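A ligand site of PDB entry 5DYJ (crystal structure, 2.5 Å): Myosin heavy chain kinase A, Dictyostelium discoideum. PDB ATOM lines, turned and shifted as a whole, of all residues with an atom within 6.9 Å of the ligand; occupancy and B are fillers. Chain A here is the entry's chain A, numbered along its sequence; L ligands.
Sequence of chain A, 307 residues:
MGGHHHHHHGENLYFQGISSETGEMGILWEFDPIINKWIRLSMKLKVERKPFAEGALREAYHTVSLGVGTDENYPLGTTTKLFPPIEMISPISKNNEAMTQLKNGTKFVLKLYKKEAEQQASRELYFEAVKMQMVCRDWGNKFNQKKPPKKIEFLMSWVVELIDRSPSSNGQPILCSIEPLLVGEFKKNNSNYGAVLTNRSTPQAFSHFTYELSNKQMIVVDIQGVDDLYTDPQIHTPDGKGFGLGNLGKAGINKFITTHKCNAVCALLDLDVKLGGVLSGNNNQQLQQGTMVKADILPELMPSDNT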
ATOM      1  N   PHE A  52      23.232 -13.789   7.320  1.00  0.00           N
ATOM      2  CA  PHE A  52      23.385 -15.222   7.584  1.00  0.00           C
ATOM      3  C   PHE A  52      23.409 -15.555   9.070  1.00  0.00           C
ATOM      4  O   PHE A  52      23.372 -16.741   9.414  1.00  0.00           O
ATOM      5  CB  PHE A  52      24.651 -15.761   6.911  1.00  0.00           C
ATOM      6  CG  PHE A  52      25.936 -15.323   7.569  1.00  0.00           C
ATOM      7  CD1 PHE A  52      26.550 -14.139   7.197  1.00  0.00           C
ATOM      8  CD2 PHE A  52      26.526 -16.107   8.551  1.00  0.00           C
ATOM      9  CE1 PHE A  52      27.737 -13.746   7.798  1.00  0.00           C
ATOM     10  CE2 PHE A  52      27.702 -15.720   9.158  1.00  0.00           C
ATOM     11  CZ  PHE A  52      28.303 -14.531   8.784  1.00  0.00           C
ATOM     12  N   ALA A  53      23.477 -14.557   9.942  1.00  0.00           N
ATOM     13  CA  ALA A  53      23.470 -14.798  11.381  1.00  0.00           C
ATOM     14  C   ALA A  53      23.069 -13.502  12.067  1.00  0.00           C
ATOM     15  O   ALA A  53      23.020 -12.436  11.459  1.00  0.00           O
ATOM     16  CB  ALA A  53      24.838 -15.274  11.869  1.00  0.00           C
ATOM     17  N   GLU A  54      22.771 -13.614  13.362  1.00  0.00           N
ATOM     18  CA  GLU A  54      22.375 -12.444  14.130  1.00  0.00           C
ATOM     19  C   GLU A  54      22.741 -12.633  15.599  1.00  0.00           C
ATOM     20  O   GLU A  54      22.706 -13.750  16.118  1.00  0.00           O
ATOM     21  CB  GLU A  54      20.879 -12.144  13.991  1.00  0.00           C
ATOM     22  CG  GLU A  54      19.966 -13.131  14.706  1.00  0.00           C
ATOM     23  CD  GLU A  54      18.529 -12.664  14.755  1.00  0.00           C
ATOM     24  OE1 GLU A  54      17.950 -12.373  13.677  1.00  0.00           O
ATOM     25  OE2 GLU A  54      17.966 -12.576  15.866  1.00  0.00           O
ATOM     26  N   GLY A  55      23.101 -11.528  16.234  1.00  0.00           N
ATOM     27  CA  GLY A  55      23.254 -11.465  17.667  1.00  0.00           C
ATOM     28  C   GLY A  55      22.151 -10.663  18.327  1.00  0.00           C
ATOM     29  O   GLY A  55      21.061 -10.477  17.764  1.00  0.00           O
ATOM     30  N   ALA A  56      22.441 -10.174  19.519  1.00  0.00           N
ATOM     31  CA  ALA A  56      21.446  -9.370  20.242  1.00  0.00           C
ATOM     32  C   ALA A  56      21.228  -8.030  19.551  1.00  0.00           C
ATOM     33  O   ALA A  56      20.083  -7.603  19.358  1.00  0.00           O
ATOM     34  CB  ALA A  56      21.884  -9.161  21.688  1.00  0.00           C
ATOM     35  N   LEU A  57      22.313  -7.366  19.146  1.00  0.00           N
ATOM     36  CA  LEU A  57      22.247  -6.008  18.626  1.00  0.00           C
ATOM     37  C   LEU A  57      22.444  -5.914  17.118  1.00  0.00           C
ATOM     38  O   LEU A  57      21.950  -4.963  16.513  1.00  0.00           O
ATOM     39  CB  LEU A  57      23.298  -5.132  19.310  1.00  0.00           C
ATOM     40  CG  LEU A  57      23.216  -5.038  20.839  1.00  0.00           C
ATOM     41  CD1 LEU A  57      24.513  -4.490  21.413  1.00  0.00           C
ATOM     42  CD2 LEU A  57      22.042  -4.164  21.255  1.00  0.00           C
ATOM     43  N   ARG A  58      23.161  -6.854  16.499  1.00  0.00           N
ATOM     44  CA  ARG A  58      23.596  -6.682  15.120  1.00  0.00           C
ATOM     45  C   ARG A  58      23.272  -7.923  14.290  1.00  0.00           C
ATOM     46  O   ARG A  58      23.016  -9.007  14.810  1.00  0.00           O
ATOM     47  CB  ARG A  58      25.093  -6.397  15.051  1.00  0.00           C
ATOM     48  CG  ARG A  58      25.507  -5.115  15.764  1.00  0.00           C
ATOM     49  CD  ARG A  58      26.995  -4.899  15.653  1.00  0.00           C
ATOM     50  NE  ARG A  58      27.728  -6.087  16.073  1.00  0.00           N
ATOM     51  CZ  ARG A  58      29.058  -6.200  16.013  1.00  0.00           C
ATOM     52  NH1 ARG A  58      29.792  -5.198  15.550  1.00  0.00           N
ATOM     53  NH2 ARG A  58      29.635  -7.321  16.411  1.00  0.00           N
ATOM     54  N   GLU A  59      23.299  -7.724  12.972  1.00  0.00           N
ATOM     55  CA  GLU A  59      23.163  -8.793  11.986  1.00  0.00           C
ATOM     56  C   GLU A  59      24.415  -8.852  11.135  1.00  0.00           C
ATOM     57  O   GLU A  59      25.065  -7.824  10.872  1.00  0.00           O
ATOM     58  CB  GLU A  59      21.930  -8.575  11.108  1.00  0.00           C
ATOM     59  CG  GLU A  59      20.607  -8.603  11.859  1.00  0.00           C
ATOM     60  CD  GLU A  59      19.413  -8.325  10.950  1.00  0.00           C
ATOM     61  OE1 GLU A  59      19.586  -7.632   9.927  1.00  0.00           O
ATOM     62  OE2 GLU A  59      18.310  -8.812  11.270  1.00  0.00           O
ATOM     63  N   ALA A  60      24.764 -10.053  10.688  1.00  0.00           N
ATOM     64  CA  ALA A  60      26.003 -10.302   9.954  1.00  0.00           C
ATOM     65  C   ALA A  60      25.694 -10.711   8.522  1.00  0.00           C
ATOM     66  O   ALA A  60      24.786 -11.511   8.278  1.00  0.00           O
ATOM     67  CB  ALA A  60      26.836 -11.390  10.644  1.00  0.00           C
ATOM     68  N   HIS A  62      27.379 -11.852   4.545  1.00  0.00           N
ATOM     69  CA  HIS A  62      28.489 -12.305   3.723  1.00  0.00           C
ATOM     70  C   HIS A  62      28.828 -11.247   2.687  1.00  0.00           C
ATOM     71  O   HIS A  62      27.927 -10.723   2.017  1.00  0.00           O
ATOM     72  CB  HIS A  62      28.163 -13.630   3.047  1.00  0.00           C
ATOM     73  CG  HIS A  62      28.365 -14.825   3.930  1.00  0.00           C
ATOM     74  ND1 HIS A  62      27.370 -15.735   4.197  1.00  0.00           N
ATOM     75  CD2 HIS A  62      29.461 -15.257   4.601  1.00  0.00           C
ATOM     76  CE1 HIS A  62      27.835 -16.679   4.988  1.00  0.00           C
ATOM     77  NE2 HIS A  62      29.105 -16.404   5.258  1.00  0.00           N
ATOM     78  N   VAL A 109      32.990 -10.548   6.401  1.00  0.00           N
ATOM     79  CA  VAL A 109      31.730 -10.391   7.113  1.00  0.00           C
ATOM     80  C   VAL A 109      31.486  -8.903   7.364  1.00  0.00           C
ATOM     81  O   VAL A 109      32.402  -8.168   7.750  1.00  0.00           O
ATOM     82  CB  VAL A 109      31.742 -11.177   8.447  1.00  0.00           C
ATOM     83  CG1 VAL A 109      30.501 -10.858   9.278  1.00  0.00           C
ATOM     84  CG2 VAL A 109      31.846 -12.662   8.184  1.00  0.00           C
ATOM     85  N   LYS A 111      28.701  -6.202   9.373  1.00  0.00           N
ATOM     86  CA  LYS A 111      27.759  -6.211  10.478  1.00  0.00           C
ATOM     87  C   LYS A 111      27.028  -4.875  10.580  1.00  0.00           C
ATOM     88  O   LYS A 111      27.664  -3.824  10.682  1.00  0.00           O
ATOM     89  CB  LYS A 111      28.471  -6.527  11.804  1.00  0.00           C
ATOM     90  CG  LYS A 111      29.077  -7.914  11.837  1.00  0.00           C
ATOM     91  CD  LYS A 111      29.652  -8.232  13.204  1.00  0.00           C
ATOM     92  CE  LYS A 111      30.355  -9.585  13.188  1.00  0.00           C
ATOM     93  NZ  LYS A 111      30.898  -9.938  14.521  1.00  0.00           N
ATOM     94  N   LEU A 155      40.633 -11.273  15.740  1.00  0.00           N
ATOM     95  CA  LEU A 155      40.589 -10.826  14.365  1.00  0.00           C
ATOM     96  C   LEU A 155      40.761  -9.314  14.264  1.00  0.00           C
ATOM     97  O   LEU A 155      40.495  -8.566  15.209  1.00  0.00           O
ATOM     98  CB  LEU A 155      39.259 -11.227  13.711  1.00  0.00           C
ATOM     99  CG  LEU A 155      38.962 -12.690  13.465  1.00  0.00           C
ATOM    100  CD1 LEU A 155      37.596 -12.846  12.806  1.00  0.00           C
ATOM    101  CD2 LEU A 155      40.047 -13.325  12.614  1.00  0.00           C
ATOM    102  N   GLU A 179      35.051  -7.480   9.263  1.00  0.00           N
ATOM    103  CA  GLU A 179      36.052  -8.331   9.886  1.00  0.00           C
ATOM    104  C   GLU A 179      36.189  -9.601   9.031  1.00  0.00           C
ATOM    105  O   GLU A 179      35.311  -9.887   8.209  1.00  0.00           O
ATOM    106  CB  GLU A 179      35.668  -8.695  11.331  1.00  0.00           C
ATOM    107  CG  GLU A 179      34.428  -9.571  11.460  1.00  0.00           C
ATOM    108  CD  GLU A 179      33.910  -9.633  12.886  1.00  0.00           C
ATOM    109  OE1 GLU A 179      33.635  -8.557  13.467  1.00  0.00           O
ATOM    110  OE2 GLU A 179      33.779 -10.751  13.425  1.00  0.00           O
ATOM    111  N   PRO A 180      37.274 -10.345   9.185  1.00  0.00           N
ATOM    112  CA  PRO A 180      37.454 -11.581   8.422  1.00  0.00           C
ATOM    113  C   PRO A 180      36.358 -12.612   8.723  1.00  0.00           C
ATOM    114  O   PRO A 180      35.670 -12.547   9.746  1.00  0.00           O
ATOM    115  CB  PRO A 180      38.827 -12.100   8.871  1.00  0.00           C
ATOM    116  CG  PRO A 180      39.539 -10.892   9.351  1.00  0.00           C
ATOM    117  CD  PRO A 180      38.491 -10.017   9.957  1.00  0.00           C
ATOM    118  N   LEU A 181      36.215 -13.560   7.809  1.00  0.00           N
ATOM    119  CA  LEU A 181      35.236 -14.625   7.947  1.00  0.00           C
ATOM    120  C   LEU A 181      35.822 -15.768   8.773  1.00  0.00           C
ATOM    121  O   LEU A 181      36.961 -16.186   8.544  1.00  0.00           O
ATOM    122  CB  LEU A 181      34.818 -15.153   6.570  1.00  0.00           C
ATOM    123  CG  LEU A 181      33.933 -16.407   6.573  1.00  0.00           C
ATOM    124  CD1 LEU A 181      32.612 -16.136   7.273  1.00  0.00           C
ATOM    125  CD2 LEU A 181      33.707 -16.902   5.161  1.00  0.00           C
ATOM    126  N   LEU A 182      35.037 -16.253   9.736  1.00  0.00           N
ATOM    127  CA  LEU A 182      35.404 -17.408  10.534  1.00  0.00           C
ATOM    128  C   LEU A 182      34.679 -18.634   9.987  1.00  0.00           C
ATOM    129  O   LEU A 182      33.457 -18.624   9.840  1.00  0.00           O
ATOM    130  CB  LEU A 182      35.035 -17.199  12.005  1.00  0.00           C
ATOM    131  CG  LEU A 182      35.843 -16.180  12.809  1.00  0.00           C
ATOM    132  CD1 LEU A 182      35.220 -15.951  14.177  1.00  0.00           C
ATOM    133  CD2 LEU A 182      37.291 -16.626  12.951  1.00  0.00           C
ATOM    134  N   VAL A 183      35.445 -19.680   9.693  1.00  0.00           N
ATOM    135  CA  VAL A 183      34.890 -20.939   9.187  1.00  0.00           C
ATOM    136  C   VAL A 183      34.995 -21.974  10.292  1.00  0.00           C
ATOM    137  O   VAL A 183      36.093 -22.244  10.810  1.00  0.00           O
ATOM    138  CB  VAL A 183      35.622 -21.403   7.915  1.00  0.00           C
ATOM    139  CG1 VAL A 183      34.890 -22.585   7.294  1.00  0.00           C
ATOM    140  CG2 VAL A 183      35.753 -20.264   6.927  1.00  0.00           C
ATOM    141  N   GLY A 184      33.856 -22.559  10.661  1.00  0.00           N
ATOM    142  CA  GLY A 184      33.776 -23.542  11.718  1.00  0.00           C
ATOM    143  C   GLY A 184      32.609 -23.241  12.628  1.00  0.00           C
ATOM    144  O   GLY A 184      31.787 -22.362  12.354  1.00  0.00           O
ATOM    145  N   PHE A 186      30.851 -21.631  15.579  1.00  0.00           N
ATOM    146  CA  PHE A 186      30.994 -20.437  16.397  1.00  0.00           C
ATOM    147  C   PHE A 186      30.446 -20.706  17.795  1.00  0.00           C
ATOM    148  O   PHE A 186      29.299 -21.155  17.941  1.00  0.00           O
ATOM    149  CB  PHE A 186      30.250 -19.278  15.738  1.00  0.00           C
ATOM    150  CG  PHE A 186      30.614 -17.924  16.268  1.00  0.00           C
ATOM    151  CD1 PHE A 186      30.040 -17.441  17.434  1.00  0.00           C
ATOM    152  CD2 PHE A 186      31.515 -17.114  15.598  1.00  0.00           C
ATOM    153  CE1 PHE A 186      30.359 -16.196  17.928  1.00  0.00           C
ATOM    154  CE2 PHE A 186      31.848 -15.858  16.078  1.00  0.00           C
ATOM    155  CZ  PHE A 186      31.270 -15.399  17.243  1.00  0.00           C
ATOM    156  N   LYS A 188      30.374 -19.237  22.032  1.00  0.00           N
ATOM    157  CA  LYS A 188      30.611 -18.202  23.042  1.00  0.00           C
ATOM    158  C   LYS A 188      31.009 -18.866  24.349  1.00  0.00           C
ATOM    159  O   LYS A 188      30.312 -19.759  24.836  1.00  0.00           O
ATOM    160  CB  LYS A 188      29.362 -17.342  23.230  1.00  0.00           C
ATOM    161  CG  LYS A 188      29.564 -16.093  24.054  1.00  0.00           C
ATOM    162  CD  LYS A 188      28.259 -15.322  24.167  1.00  0.00           C
ATOM    163  CE  LYS A 188      28.506 -13.881  24.559  1.00  0.00           C
ATOM    164  NZ  LYS A 188      27.247 -13.097  24.656  1.00  0.00           N
ATOM    165  N   GLN A 224      34.484 -15.143  22.456  1.00  0.00           N
ATOM    166  CA  GLN A 224      33.674 -15.936  21.546  1.00  0.00           C
ATOM    167  C   GLN A 224      34.350 -15.996  20.175  1.00  0.00           C
ATOM    168  O   GLN A 224      35.125 -15.109  19.807  1.00  0.00           O
ATOM    169  CB  GLN A 224      32.265 -15.365  21.412  1.00  0.00           C
ATOM    170  CG  GLN A 224      32.246 -13.904  20.982  1.00  0.00           C
ATOM    171  CD  GLN A 224      30.852 -13.307  20.964  1.00  0.00           C
ATOM    172  OE1 GLN A 224      29.905 -13.937  20.491  1.00  0.00           O
ATOM    173  NE2 GLN A 224      30.729 -12.091  21.476  1.00  0.00           N
ATOM    174  N   VAL A 226      35.545 -19.002  16.814  1.00  0.00           N
ATOM    175  CA  VAL A 226      35.738 -20.363  16.314  1.00  0.00           C
ATOM    176  C   VAL A 226      37.144 -20.804  16.704  1.00  0.00           C
ATOM    177  O   VAL A 226      38.125 -20.138  16.340  1.00  0.00           O
ATOM    178  CB  VAL A 226      35.536 -20.454  14.801  1.00  0.00           C
ATOM    179  CG1 VAL A 226      35.881 -21.858  14.311  1.00  0.00           C
ATOM    180  CG2 VAL A 226      34.101 -20.100  14.433  1.00  0.00           C
ATOM    181  N   THR A 231      36.430 -12.980  18.286  1.00  0.00           N
ATOM    182  CA  THR A 231      35.936 -11.699  17.811  1.00  0.00           C
ATOM    183  C   THR A 231      34.867 -11.196  18.777  1.00  0.00           C
ATOM    184  O   THR A 231      34.432 -11.922  19.673  1.00  0.00           O
ATOM    185  CB  THR A 231      35.384 -11.802  16.381  1.00  0.00           C
ATOM    186  OG1 THR A 231      35.249 -10.490  15.812  1.00  0.00           O
ATOM    187  CG2 THR A 231      34.031 -12.488  16.371  1.00  0.00           C
ATOM    188  N   ASP A 232      34.479  -9.944  18.598  1.00  0.00           N
ATOM    189  CA  ASP A 232      33.471  -9.284  19.434  1.00  0.00           C
ATOM    190  C   ASP A 232      33.698  -9.429  20.942  1.00  0.00           C
ATOM    191  O   ASP A 232      32.809  -9.878  21.659  1.00  0.00           O
ATOM    192  CB  ASP A 232      32.085  -9.787  19.058  1.00  0.00           C
ATOM    193  CG  ASP A 232      31.597  -9.257  17.737  1.00  0.00           C
ATOM    194  OD1 ASP A 232      31.322  -8.037  17.663  1.00  0.00           O
ATOM    195  OD2 ASP A 232      31.493 -10.037  16.771  1.00  0.00           O
HETATM  196  P1  LIG L   1      27.537 -10.806  17.109  1.00  0.00           P
HETATM  197  O1  LIG L   1      26.164 -10.192  16.992  1.00  0.00           O
HETATM  198  O2  LIG L   1      27.916 -11.195  18.518  1.00  0.00           O
HETATM  199  O3  LIG L   1      28.599 -10.064  16.329  1.00  0.00           O
HETATM  200  O4  LIG L   1      27.433 -12.214  16.377  1.00  0.00           O
HETATM  201  C1  LIG L   1      26.280 -12.600  15.653  1.00  0.00           C
HETATM  202  C2  LIG L   1      26.472 -13.972  15.048  1.00  0.00           C
HETATM  203  O5  LIG L   1      27.179 -13.831  13.793  1.00  0.00           O
HETATM  204  C3  LIG L   1      27.327 -14.924  15.869  1.00  0.00           C
HETATM  205  O6  LIG L   1      26.572 -15.634  16.834  1.00  0.00           O
HETATM  206  C4  LIG L   1      27.982 -15.820  14.828  1.00  0.00           C
HETATM  207  O7  LIG L   1      27.124 -16.910  14.495  1.00  0.00           O
HETATM  208  C5  LIG L   1      28.075 -14.892  13.606  1.00  0.00           C
HETATM  209  N1  LIG L   1      29.420 -14.319  13.430  1.00  0.00           N
HETATM  210  C6  LIG L   1      29.909 -13.270  14.120  1.00  0.00           C
HETATM  211  N2  LIG L   1      31.171 -12.962  13.720  1.00  0.00           N
HETATM  212  C7  LIG L   1      31.503 -13.820  12.744  1.00  0.00           C
HETATM  213  C8  LIG L   1      32.688 -14.063  11.887  1.00  0.00           C
HETATM  214  N3  LIG L   1      33.798 -13.283  11.996  1.00  0.00           N
HETATM  215  N4  LIG L   1      32.632 -15.071  10.992  1.00  0.00           N
HETATM  216  C9  LIG L   1      31.534 -15.845  10.877  1.00  0.00           C
HETATM  217  N5  LIG L   1      30.429 -15.690  11.618  1.00  0.00           N
HETATM  218  C10 LIG L   1      30.356 -14.713  12.554  1.00  0.00           C
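The backbone NH (N) of Gly 55 sits close to an oxygen (O1) of the ligand (3.4 Å).
A nitrogen (N4) of the ligand sits at hydrogen-bond distance from the backbone NH (N) of Leu 182.
NZ of Lys 111 lies within salt-bridge range of O3 of the ligand (2.9 Å).
O of Pro 180 lies within hydrogen-bond range of N3 of the ligand (3.0 Å).
OD2 of Asp 232 lies close to O3 of the ligand, 2.9 Å away.
NH2 of Arg 58 is in salt-bridge range of O3 of the ligand, at 2.9 Å.
The side-chain carboxylate (OE2) of Glu 179 is in hydrogen-bond range of a nitrogen (N3) of the ligand (2.9 Å).
The backbone NH (N) of Ala 60 sits at hydrogen-bond distance from the backbone carbonyl oxygen (O) of Ala 53, at 3.1 Å.
The side-chain carboxylate (OD1) of Asp 232 is in salt-bridge range of the side-chain amino group (NZ) of Lys 111 (3.7 Å).
The backbone carbonyl oxygen (O) of Gln 224 sits at hydrogen-bond distance from the backbone NH (N) of Thr 231, at 2.9 Å.
The backbone carbonyl oxygen (O) of Asp 232 sits at hydrogen-bond distance from the side-chain amide nitrogen (NE2) of Gln 224 (3.0 Å).
The backbone carbonyl oxygen (O) of Ala 60 is in hydrogen-bond range of the backbone NH (N) of Phe 52, at 2.9 Å.
The backbone carbonyl oxygen (O) of Glu 179 sits at hydrogen-bond distance from the backbone NH (N) of Val 109, at 3.0 Å.
OD2 of Asp 232 lies within salt-bridge range of NH2 of Arg 58 (3.3 Å).
OG1 of Thr 231 sits at hydrogen-bond distance from OE2 of Glu 179 (2.8 Å).
Merely in contact with the ligand: Ala 53, Glu 54, Phe 186, Phe 52, Leu 181, Val 109, Leu 155, Gln 224, Thr 231 and Ala 60.
Within 4 Å of the ligand: Phe 52, Ala 53, Glu 54, Gly 55, Arg 58, Ala 60, Val 109, Lys 111, Leu 155, Glu 179, Pro 180, Leu 181, Leu 182, Phe 186, Gln 224, Thr 231 and Asp 232.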
